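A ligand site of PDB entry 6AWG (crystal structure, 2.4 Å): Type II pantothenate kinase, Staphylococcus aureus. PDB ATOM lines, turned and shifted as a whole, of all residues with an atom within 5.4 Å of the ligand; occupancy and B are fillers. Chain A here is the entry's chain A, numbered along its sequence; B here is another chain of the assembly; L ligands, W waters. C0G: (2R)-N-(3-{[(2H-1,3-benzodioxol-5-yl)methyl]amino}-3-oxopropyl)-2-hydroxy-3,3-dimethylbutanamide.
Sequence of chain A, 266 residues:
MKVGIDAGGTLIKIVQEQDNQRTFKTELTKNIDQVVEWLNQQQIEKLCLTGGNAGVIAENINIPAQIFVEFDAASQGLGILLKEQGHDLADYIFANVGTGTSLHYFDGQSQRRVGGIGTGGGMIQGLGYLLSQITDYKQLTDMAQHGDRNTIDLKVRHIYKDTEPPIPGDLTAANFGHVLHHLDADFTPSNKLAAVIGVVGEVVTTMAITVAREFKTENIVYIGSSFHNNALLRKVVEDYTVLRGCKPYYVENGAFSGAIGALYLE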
ATOM      1  N   VAL A 156     -18.688 -11.589  21.409  1.00  0.00           N
ATOM      2  CA  VAL A 156     -19.467 -11.252  20.262  1.00  0.00           C
ATOM      3  C   VAL A 156     -20.845 -10.656  20.628  1.00  0.00           C
ATOM      4  O   VAL A 156     -21.313  -9.770  19.998  1.00  0.00           O
ATOM      5  CB  VAL A 156     -19.578 -12.485  19.348  1.00  0.00           C
ATOM      6  CG1 VAL A 156     -20.579 -12.308  18.261  1.00  0.00           C
ATOM      7  CG2 VAL A 156     -18.244 -12.874  18.799  1.00  0.00           C
ATOM      8  N   ILE A 159     -20.747  -6.934  21.475  1.00  0.00           N
ATOM      9  CA  ILE A 159     -20.692  -6.127  20.315  1.00  0.00           C
ATOM     10  C   ILE A 159     -22.040  -6.085  19.613  1.00  0.00           C
ATOM     11  O   ILE A 159     -22.488  -5.046  19.280  1.00  0.00           O
ATOM     12  CB  ILE A 159     -19.604  -6.611  19.341  1.00  0.00           C
ATOM     13  CG1 ILE A 159     -18.208  -6.471  19.956  1.00  0.00           C
ATOM     14  CG2 ILE A 159     -19.720  -5.914  18.016  1.00  0.00           C
ATOM     15  CD1 ILE A 159     -17.069  -6.746  19.012  1.00  0.00           C
ATOM     16  N   TYR A 160     -22.682  -7.233  19.448  1.00  0.00           N
ATOM     17  CA  TYR A 160     -23.981  -7.326  18.775  1.00  0.00           C
ATOM     18  C   TYR A 160     -25.170  -7.043  19.669  1.00  0.00           C
ATOM     19  O   TYR A 160     -26.254  -6.916  19.182  1.00  0.00           O
ATOM     20  CB  TYR A 160     -24.124  -8.668  18.053  1.00  0.00           C
ATOM     21  CG  TYR A 160     -23.603  -8.539  16.648  1.00  0.00           C
ATOM     22  CD1 TYR A 160     -22.240  -8.547  16.381  1.00  0.00           C
ATOM     23  CD2 TYR A 160     -24.479  -8.317  15.579  1.00  0.00           C
ATOM     24  CE1 TYR A 160     -21.762  -8.354  15.102  1.00  0.00           C
ATOM     25  CE2 TYR A 160     -23.992  -8.118  14.292  1.00  0.00           C
ATOM     26  CZ  TYR A 160     -22.620  -8.127  14.069  1.00  0.00           C
ATOM     27  OH  TYR A 160     -22.135  -7.978  12.789  1.00  0.00           O
ATOM     28  N   PRO A 166     -23.561 -12.775  13.649  1.00  0.00           N
ATOM     29  CA  PRO A 166     -23.185 -13.617  12.514  1.00  0.00           C
ATOM     30  C   PRO A 166     -22.300 -14.822  12.877  1.00  0.00           C
ATOM     31  O   PRO A 166     -22.031 -15.682  11.998  1.00  0.00           O
ATOM     32  CB  PRO A 166     -22.424 -12.650  11.625  1.00  0.00           C
ATOM     33  CG  PRO A 166     -21.729 -11.770  12.598  1.00  0.00           C
ATOM     34  CD  PRO A 166     -22.668 -11.609  13.768  1.00  0.00           C
ATOM     35  N   ILE A 167     -21.808 -14.863  14.116  1.00  0.00           N
ATOM     36  CA  ILE A 167     -21.147 -16.032  14.688  1.00  0.00           C
ATOM     37  C   ILE A 167     -21.592 -16.138  16.136  1.00  0.00           C
ATOM     38  O   ILE A 167     -22.011 -15.156  16.724  1.00  0.00           O
ATOM     39  CB  ILE A 167     -19.599 -15.951  14.585  1.00  0.00           C
ATOM     40  CG1 ILE A 167     -19.016 -14.712  15.266  1.00  0.00           C
ATOM     41  CG2 ILE A 167     -19.184 -15.920  13.120  1.00  0.00           C
ATOM     42  CD1 ILE A 167     -17.541 -14.851  15.548  1.00  0.00           C
ATOM     43  N   ASP A 170     -21.321 -16.162  22.396  1.00  0.00           N
ATOM     44  CA  ASP A 170     -20.396 -16.455  23.526  1.00  0.00           C
ATOM     45  C   ASP A 170     -18.878 -16.451  23.111  1.00  0.00           C
ATOM     46  O   ASP A 170     -18.009 -16.428  23.959  1.00  0.00           O
ATOM     47  CB  ASP A 170     -20.774 -17.791  24.169  1.00  0.00           C
ATOM     48  CG  ASP A 170     -20.090 -18.001  25.501  1.00  0.00           C
ATOM     49  OD1 ASP A 170     -20.075 -17.068  26.327  1.00  0.00           O
ATOM     50  OD2 ASP A 170     -19.559 -19.108  25.750  1.00  0.00           O
ATOM     51  N   LEU A 171     -18.591 -16.402  21.809  1.00  0.00           N
ATOM     52  CA  LEU A 171     -17.220 -16.426  21.340  1.00  0.00           C
ATOM     53  C   LEU A 171     -16.503 -15.139  21.735  1.00  0.00           C
ATOM     54  O   LEU A 171     -17.151 -14.102  21.964  1.00  0.00           O
ATOM     55  CB  LEU A 171     -17.165 -16.622  19.827  1.00  0.00           C
ATOM     56  CG  LEU A 171     -17.719 -17.955  19.310  1.00  0.00           C
ATOM     57  CD1 LEU A 171     -17.802 -17.957  17.781  1.00  0.00           C
ATOM     58  CD2 LEU A 171     -16.919 -19.157  19.791  1.00  0.00           C
ATOM     59  N   THR A 172     -15.182 -15.227  21.880  1.00  0.00           N
ATOM     60  CA  THR A 172     -14.333 -14.062  22.136  1.00  0.00           C
ATOM     61  C   THR A 172     -14.264 -13.259  20.860  1.00  0.00           C
ATOM     62  O   THR A 172     -13.898 -13.761  19.816  1.00  0.00           O
ATOM     63  CB  THR A 172     -12.887 -14.441  22.495  1.00  0.00           C
ATOM     64  OG1 THR A 172     -12.898 -15.332  23.608  1.00  0.00           O
ATOM     65  CG2 THR A 172     -12.084 -13.191  22.877  1.00  0.00           C
ATOM     66  N   ALA A 173     -14.694 -12.016  20.941  1.00  0.00           N
ATOM     67  CA  ALA A 173     -14.593 -11.113  19.830  1.00  0.00           C
ATOM     68  C   ALA A 173     -13.259 -10.401  19.857  1.00  0.00           C
ATOM     69  O   ALA A 173     -12.697 -10.140  18.792  1.00  0.00           O
ATOM     70  CB  ALA A 173     -15.687 -10.099  19.885  1.00  0.00           C
ATOM     71  N   ALA A 174     -12.767 -10.075  21.053  1.00  0.00           N
ATOM     72  CA  ALA A 174     -11.614  -9.190  21.237  1.00  0.00           C
ATOM     73  C   ALA A 174     -10.967  -9.425  22.603  1.00  0.00           C
ATOM     74  O   ALA A 174     -11.488  -8.981  23.691  1.00  0.00           O
ATOM     75  CB  ALA A 174     -12.024  -7.740  21.087  1.00  0.00           C
ATOM     76  N   GLU A 202      -6.140 -19.280  22.582  1.00  0.00           N
ATOM     77  CA  GLU A 202      -7.067 -19.041  21.467  1.00  0.00           C
ATOM     78  C   GLU A 202      -6.312 -18.877  20.172  1.00  0.00           C
ATOM     79  O   GLU A 202      -6.734 -19.383  19.138  1.00  0.00           O
ATOM     80  CB  GLU A 202      -7.955 -17.814  21.718  1.00  0.00           C
ATOM     81  CG  GLU A 202      -8.898 -17.979  22.896  1.00  0.00           C
ATOM     82  CD  GLU A 202      -9.894 -16.833  23.119  1.00  0.00           C
ATOM     83  OE1 GLU A 202      -9.888 -15.783  22.431  1.00  0.00           O
ATOM     84  OE2 GLU A 202     -10.728 -16.997  24.009  1.00  0.00           O
ATOM     85  N   THR A 206      -6.653 -21.469  17.183  1.00  0.00           N
ATOM     86  CA  THR A 206      -7.149 -20.885  15.894  1.00  0.00           C
ATOM     87  C   THR A 206      -6.281 -21.259  14.693  1.00  0.00           C
ATOM     88  O   THR A 206      -6.765 -21.674  13.642  1.00  0.00           O
ATOM     89  CB  THR A 206      -7.235 -19.345  15.948  1.00  0.00           C
ATOM     90  OG1 THR A 206      -8.120 -18.965  17.005  1.00  0.00           O
ATOM     91  CG2 THR A 206      -7.755 -18.790  14.599  1.00  0.00           C
ATOM     92  N   VAL A 236      -8.729 -24.080  27.676  1.00  0.00           N
ATOM     93  CA  VAL A 236      -8.972 -23.109  26.594  1.00  0.00           C
ATOM     94  C   VAL A 236      -8.785 -23.773  25.222  1.00  0.00           C
ATOM     95  O   VAL A 236      -9.630 -23.673  24.325  1.00  0.00           O
ATOM     96  CB  VAL A 236      -8.029 -21.873  26.747  1.00  0.00           C
ATOM     97  CG1 VAL A 236      -8.019 -21.016  25.503  1.00  0.00           C
ATOM     98  CG2 VAL A 236      -8.398 -21.028  27.985  1.00  0.00           C
ATOM     99  N   TYR A 240     -12.142 -24.981  22.659  1.00  0.00           N
ATOM    100  CA  TYR A 240     -12.275 -24.386  21.349  1.00  0.00           C
ATOM    101  C   TYR A 240     -11.942 -25.351  20.195  1.00  0.00           C
ATOM    102  O   TYR A 240     -12.474 -25.197  19.076  1.00  0.00           O
ATOM    103  CB  TYR A 240     -11.441 -23.105  21.259  1.00  0.00           C
ATOM    104  CG  TYR A 240     -11.811 -22.289  20.065  1.00  0.00           C
ATOM    105  CD1 TYR A 240     -13.076 -21.683  19.978  1.00  0.00           C
ATOM    106  CD2 TYR A 240     -10.941 -22.133  19.011  1.00  0.00           C
ATOM    107  CE1 TYR A 240     -13.421 -20.916  18.882  1.00  0.00           C
ATOM    108  CE2 TYR A 240     -11.276 -21.368  17.902  1.00  0.00           C
ATOM    109  CZ  TYR A 240     -12.513 -20.751  17.865  1.00  0.00           C
ATOM    110  OH  TYR A 240     -12.867 -19.999  16.773  1.00  0.00           O
ATOM    111  N   GLU B  70     -22.803  -7.509   8.157  1.00  0.00           N
ATOM    112  CA  GLU B  70     -21.541  -6.754   8.040  1.00  0.00           C
ATOM    113  C   GLU B  70     -20.528  -7.358   7.096  1.00  0.00           C
ATOM    114  O   GLU B  70     -19.878  -6.636   6.352  1.00  0.00           O
ATOM    115  CB  GLU B  70     -20.967  -6.330   9.398  1.00  0.00           C
ATOM    116  CG  GLU B  70     -20.236  -7.339  10.246  1.00  0.00           C
ATOM    117  CD  GLU B  70     -19.272  -6.651  11.229  1.00  0.00           C
ATOM    118  OE1 GLU B  70     -18.167  -6.217  10.789  1.00  0.00           O
ATOM    119  OE2 GLU B  70     -19.631  -6.522  12.436  1.00  0.00           O
ATOM    120  N   PHE B  71     -20.463  -8.676   7.048  1.00  0.00           N
ATOM    121  CA  PHE B  71     -19.503  -9.348   6.194  1.00  0.00           C
ATOM    122  C   PHE B  71     -19.801  -9.129   4.724  1.00  0.00           C
ATOM    123  O   PHE B  71     -18.890  -8.889   3.928  1.00  0.00           O
ATOM    124  CB  PHE B  71     -19.393 -10.850   6.499  1.00  0.00           C
ATOM    125  CG  PHE B  71     -19.102 -11.165   7.952  1.00  0.00           C
ATOM    126  CD1 PHE B  71     -18.342 -10.285   8.774  1.00  0.00           C
ATOM    127  CD2 PHE B  71     -19.559 -12.351   8.507  1.00  0.00           C
ATOM    128  CE1 PHE B  71     -18.067 -10.599  10.115  1.00  0.00           C
ATOM    129  CE2 PHE B  71     -19.316 -12.651   9.834  1.00  0.00           C
ATOM    130  CZ  PHE B  71     -18.557 -11.766  10.647  1.00  0.00           C
ATOM    131  N   THR B  99     -12.237  -4.050  16.214  1.00  0.00           N
ATOM    132  CA  THR B  99     -12.080  -4.265  17.635  1.00  0.00           C
ATOM    133  C   THR B  99     -11.458  -5.637  17.806  1.00  0.00           C
ATOM    134  O   THR B  99     -10.550  -5.821  18.644  1.00  0.00           O
ATOM    135  CB  THR B  99     -13.415  -4.198  18.375  1.00  0.00           C
ATOM    136  OG1 THR B  99     -14.073  -2.967  18.051  1.00  0.00           O
ATOM    137  CG2 THR B  99     -13.179  -4.195  19.841  1.00  0.00           C
ATOM    138  N   GLY B 100     -11.990  -6.567  17.015  1.00  0.00           N
ATOM    139  CA  GLY B 100     -11.433  -7.886  16.753  1.00  0.00           C
ATOM    140  C   GLY B 100     -11.224  -8.101  15.257  1.00  0.00           C
ATOM    141  O   GLY B 100     -11.701  -7.328  14.431  1.00  0.00           O
ATOM    142  N   THR B 101     -10.507  -9.179  14.911  1.00  0.00           N
ATOM    143  CA  THR B 101     -10.179  -9.469  13.506  1.00  0.00           C
ATOM    144  C   THR B 101     -11.024 -10.578  12.849  1.00  0.00           C
ATOM    145  O   THR B 101     -11.235 -11.649  13.410  1.00  0.00           O
ATOM    146  CB  THR B 101      -8.692  -9.739  13.354  1.00  0.00           C
ATOM    147  OG1 THR B 101      -7.979  -8.615  13.923  1.00  0.00           O
ATOM    148  CG2 THR B 101      -8.305  -9.933  11.873  1.00  0.00           C
ATOM    149  N   SER B 102     -11.524 -10.273  11.650  1.00  0.00           N
ATOM    150  CA  SER B 102     -12.241 -11.242  10.835  1.00  0.00           C
ATOM    151  C   SER B 102     -11.601 -11.390   9.469  1.00  0.00           C
ATOM    152  O   SER B 102     -11.278 -10.388   8.855  1.00  0.00           O
ATOM    153  CB  SER B 102     -13.708 -10.831  10.687  1.00  0.00           C
ATOM    154  OG  SER B 102     -14.447 -11.825  10.018  1.00  0.00           O
ATOM    155  N   ARG B 113     -16.353 -16.112   4.911  1.00  0.00           N
ATOM    156  CA  ARG B 113     -15.518 -16.068   6.134  1.00  0.00           C
ATOM    157  C   ARG B 113     -14.718 -17.336   6.251  1.00  0.00           C
ATOM    158  O   ARG B 113     -15.286 -18.401   6.252  1.00  0.00           O
ATOM    159  CB  ARG B 113     -16.340 -15.897   7.406  1.00  0.00           C
ATOM    160  CG  ARG B 113     -15.516 -15.416   8.603  1.00  0.00           C
ATOM    161  CD  ARG B 113     -16.429 -14.755   9.641  1.00  0.00           C
ATOM    162  NE  ARG B 113     -15.750 -14.167  10.810  1.00  0.00           N
ATOM    163  CZ  ARG B 113     -15.252 -14.847  11.832  1.00  0.00           C
ATOM    164  NH1 ARG B 113     -15.289 -16.172  11.831  1.00  0.00           N
ATOM    165  NH2 ARG B 113     -14.677 -14.207  12.852  1.00  0.00           N
ATOM    166  N   GLY B 115     -11.981 -17.291   8.663  1.00  0.00           N
ATOM    167  CA  GLY B 115     -11.675 -17.345  10.084  1.00  0.00           C
ATOM    168  C   GLY B 115     -11.691 -16.025  10.800  1.00  0.00           C
ATOM    169  O   GLY B 115     -12.120 -15.005  10.274  1.00  0.00           O
ATOM    170  N   GLY B 116     -11.212 -16.036  12.021  1.00  0.00           N
ATOM    171  CA  GLY B 116     -11.164 -14.826  12.812  1.00  0.00           C
ATOM    172  C   GLY B 116     -10.349 -15.011  14.050  1.00  0.00           C
ATOM    173  O   GLY B 116     -10.003 -16.120  14.419  1.00  0.00           O
ATOM    174  N   ILE B 117     -10.049 -13.912  14.715  1.00  0.00           N
ATOM    175  CA  ILE B 117      -9.224 -13.936  15.891  1.00  0.00           C
ATOM    176  C   ILE B 117      -9.458 -12.662  16.694  1.00  0.00           C
ATOM    177  O   ILE B 117      -9.642 -11.589  16.141  1.00  0.00           O
ATOM    178  CB  ILE B 117      -7.709 -14.208  15.499  1.00  0.00           C
ATOM    179  CG1 ILE B 117      -6.790 -14.405  16.704  1.00  0.00           C
ATOM    180  CG2 ILE B 117      -7.139 -13.096  14.604  1.00  0.00           C
ATOM    181  CD1 ILE B 117      -7.070 -15.624  17.562  1.00  0.00           C
ATOM    182  N   GLY B 118      -9.431 -12.793  18.007  1.00  0.00           N
ATOM    183  CA  GLY B 118      -9.632 -11.630  18.897  1.00  0.00           C
ATOM    184  C   GLY B 118      -8.393 -10.788  19.122  1.00  0.00           C
ATOM    185  O   GLY B 118      -8.372 -10.002  20.073  1.00  0.00           O
HETATM  186  C02 C0G L   1     -17.291  -8.068  14.959  1.00  0.00           C
HETATM  187  C03 C0G L   1     -16.702  -9.513  14.854  1.00  0.00           C
HETATM  188  C04 C0G L   1     -17.252 -10.120  13.545  1.00  0.00           C
HETATM  189  C25 C0G L   1     -17.119 -10.342  16.097  1.00  0.00           C
HETATM  190  C05 C0G L   1     -15.154  -9.448  14.822  1.00  0.00           C
HETATM  191  O24 C0G L   1     -14.694  -8.659  15.937  1.00  0.00           O
HETATM  192  C06 C0G L   1     -14.528 -10.887  14.821  1.00  0.00           C
HETATM  193  O23 C0G L   1     -14.674 -11.650  13.876  1.00  0.00           O
HETATM  194  N07 C0G L   1     -13.919 -11.238  15.968  1.00  0.00           N
HETATM  195  C08 C0G L   1     -13.192 -12.506  16.190  1.00  0.00           C
HETATM  196  C09 C0G L   1     -14.135 -13.632  16.492  1.00  0.00           C
HETATM  197  C10 C0G L   1     -13.325 -14.916  16.385  1.00  0.00           C
HETATM  198  O22 C0G L   1     -13.279 -15.513  15.316  1.00  0.00           O
HETATM  199  N11 C0G L   1     -12.721 -15.295  17.495  1.00  0.00           N
HETATM  200  C12 C0G L   1     -11.829 -16.418  17.583  1.00  0.00           C
HETATM  201  C13 C0G L   1     -11.974 -17.167  18.801  1.00  0.00           C
HETATM  202  C21 C0G L   1     -13.067 -17.210  19.687  1.00  0.00           C
HETATM  203  C17 C0G L   1     -13.040 -18.008  20.769  1.00  0.00           C
HETATM  204  O18 C0G L   1     -13.980 -18.144  21.724  1.00  0.00           O
HETATM  205  C19 C0G L   1     -13.335 -18.939  22.746  1.00  0.00           C
HETATM  206  O20 C0G L   1     -12.162 -19.535  22.151  1.00  0.00           O
HETATM  207  C16 C0G L   1     -11.996 -18.812  21.032  1.00  0.00           C
HETATM  208  C15 C0G L   1     -10.955 -18.847  20.231  1.00  0.00           C
HETATM  209  C14 C0G L   1     -10.933 -18.032  19.111  1.00  0.00           C
HETATM  210  O   HOH W   1     -15.945  -8.018  11.116  1.00  0.00           O
HETATM  211  O   HOH W   2     -15.667 -17.865  24.305  1.00  0.00           O
HETATM  212  O   HOH W   3     -14.460  -6.229  15.012  1.00  0.00           O
HETATM  213  O   HOH W   4     -11.403 -19.020  25.602  1.00  0.00           O
HETATM  214  O   HOH W   5     -17.010  -4.852  15.142  1.00  0.00           O
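Water W3 lies within hydrogen-bond range of O24 of the ligand (2.6 Å), O of Gly 100 of chain B (3.0 Å) and N of Thr 99 of chain B (3.3 Å).
Water W2 lies within hydrogen-bond range of the backbone carbonyl oxygen (O) of Asp 170 and an oxygen (O18) of the ligand.
O23 of the ligand sits at hydrogen-bond distance from NH2 of Arg 113 of chain B, at 2.8 Å.
The backbone NH (N) of Thr 172 is in hydrogen-bond range of an oxygen (O18) of the ligand.
The backbone carbonyl oxygen (O) of Thr 172 lies within hydrogen-bond range of a nitrogen (N11) of the ligand (3.0 Å).
The backbone carbonyl oxygen (O) of Ala 173 lies within hydrogen-bond range of a nitrogen (N07) of the ligand.
NE of Arg 113 of chain B lies within hydrogen-bond range of OG of Ser 102 of chain B, 2.8 Å away.
The side-chain hydroxyl (OG1) of Thr 172 is in hydrogen-bond range of the side-chain carboxylate (OE2) of Glu 202 (2.8 Å).
The backbone carbonyl oxygen (O) of Glu 202 lies within hydrogen-bond range of the side-chain hydroxyl (OG1) of Thr 206.
The backbone NH (N) of Thr 101 of chain B sits at hydrogen-bond distance from the backbone carbonyl oxygen (O) of Ile 117 of chain B (2.8 Å).
O of Leu 171 lies within hydrogen-bond range of N of Val 156 (3.0 Å).
The side-chain hydroxyl (OH) of Tyr 160 lies within hydrogen-bond range of the side-chain carboxylate (OE2) of Glu 70 of chain B, at 2.9 Å.
OE2 of Glu 202 sits close to O20 of the ligand, 3.5 Å away.
O of Thr 101 of chain B sits close to O23 of the ligand.
The backbone carbonyl oxygen (O) of Gly 116 of chain B lies close to an oxygen (O22) of the ligand (3.5 Å).
Val 156 touches the ligand.
Ile 167 touches the ligand (CD1 to C09, 3.7 Å).
CD2 of Leu 171 touches O18 of the ligand, 3.7 Å away.
Thr 206 touches the ligand.
CD1 of Tyr 240 touches O20 of the ligand (3.2 Å).
OE2 of Glu 70 of chain B touches C02 of the ligand (3.8 Å).
Phe 71 of chain B touches the ligand.
CA of Gly 100 of chain B touches O24 of the ligand, 3.4 Å away.
Ser 102 of chain B touches the ligand (CB to O23, 3.4 Å).
Ile 117 of chain B touches the ligand.
Hydrophobic or aromatic side chains within 4 Å of the ligand: Val 156, Ile 167, Leu 171, Tyr 240 and Phe 71 of chain B.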
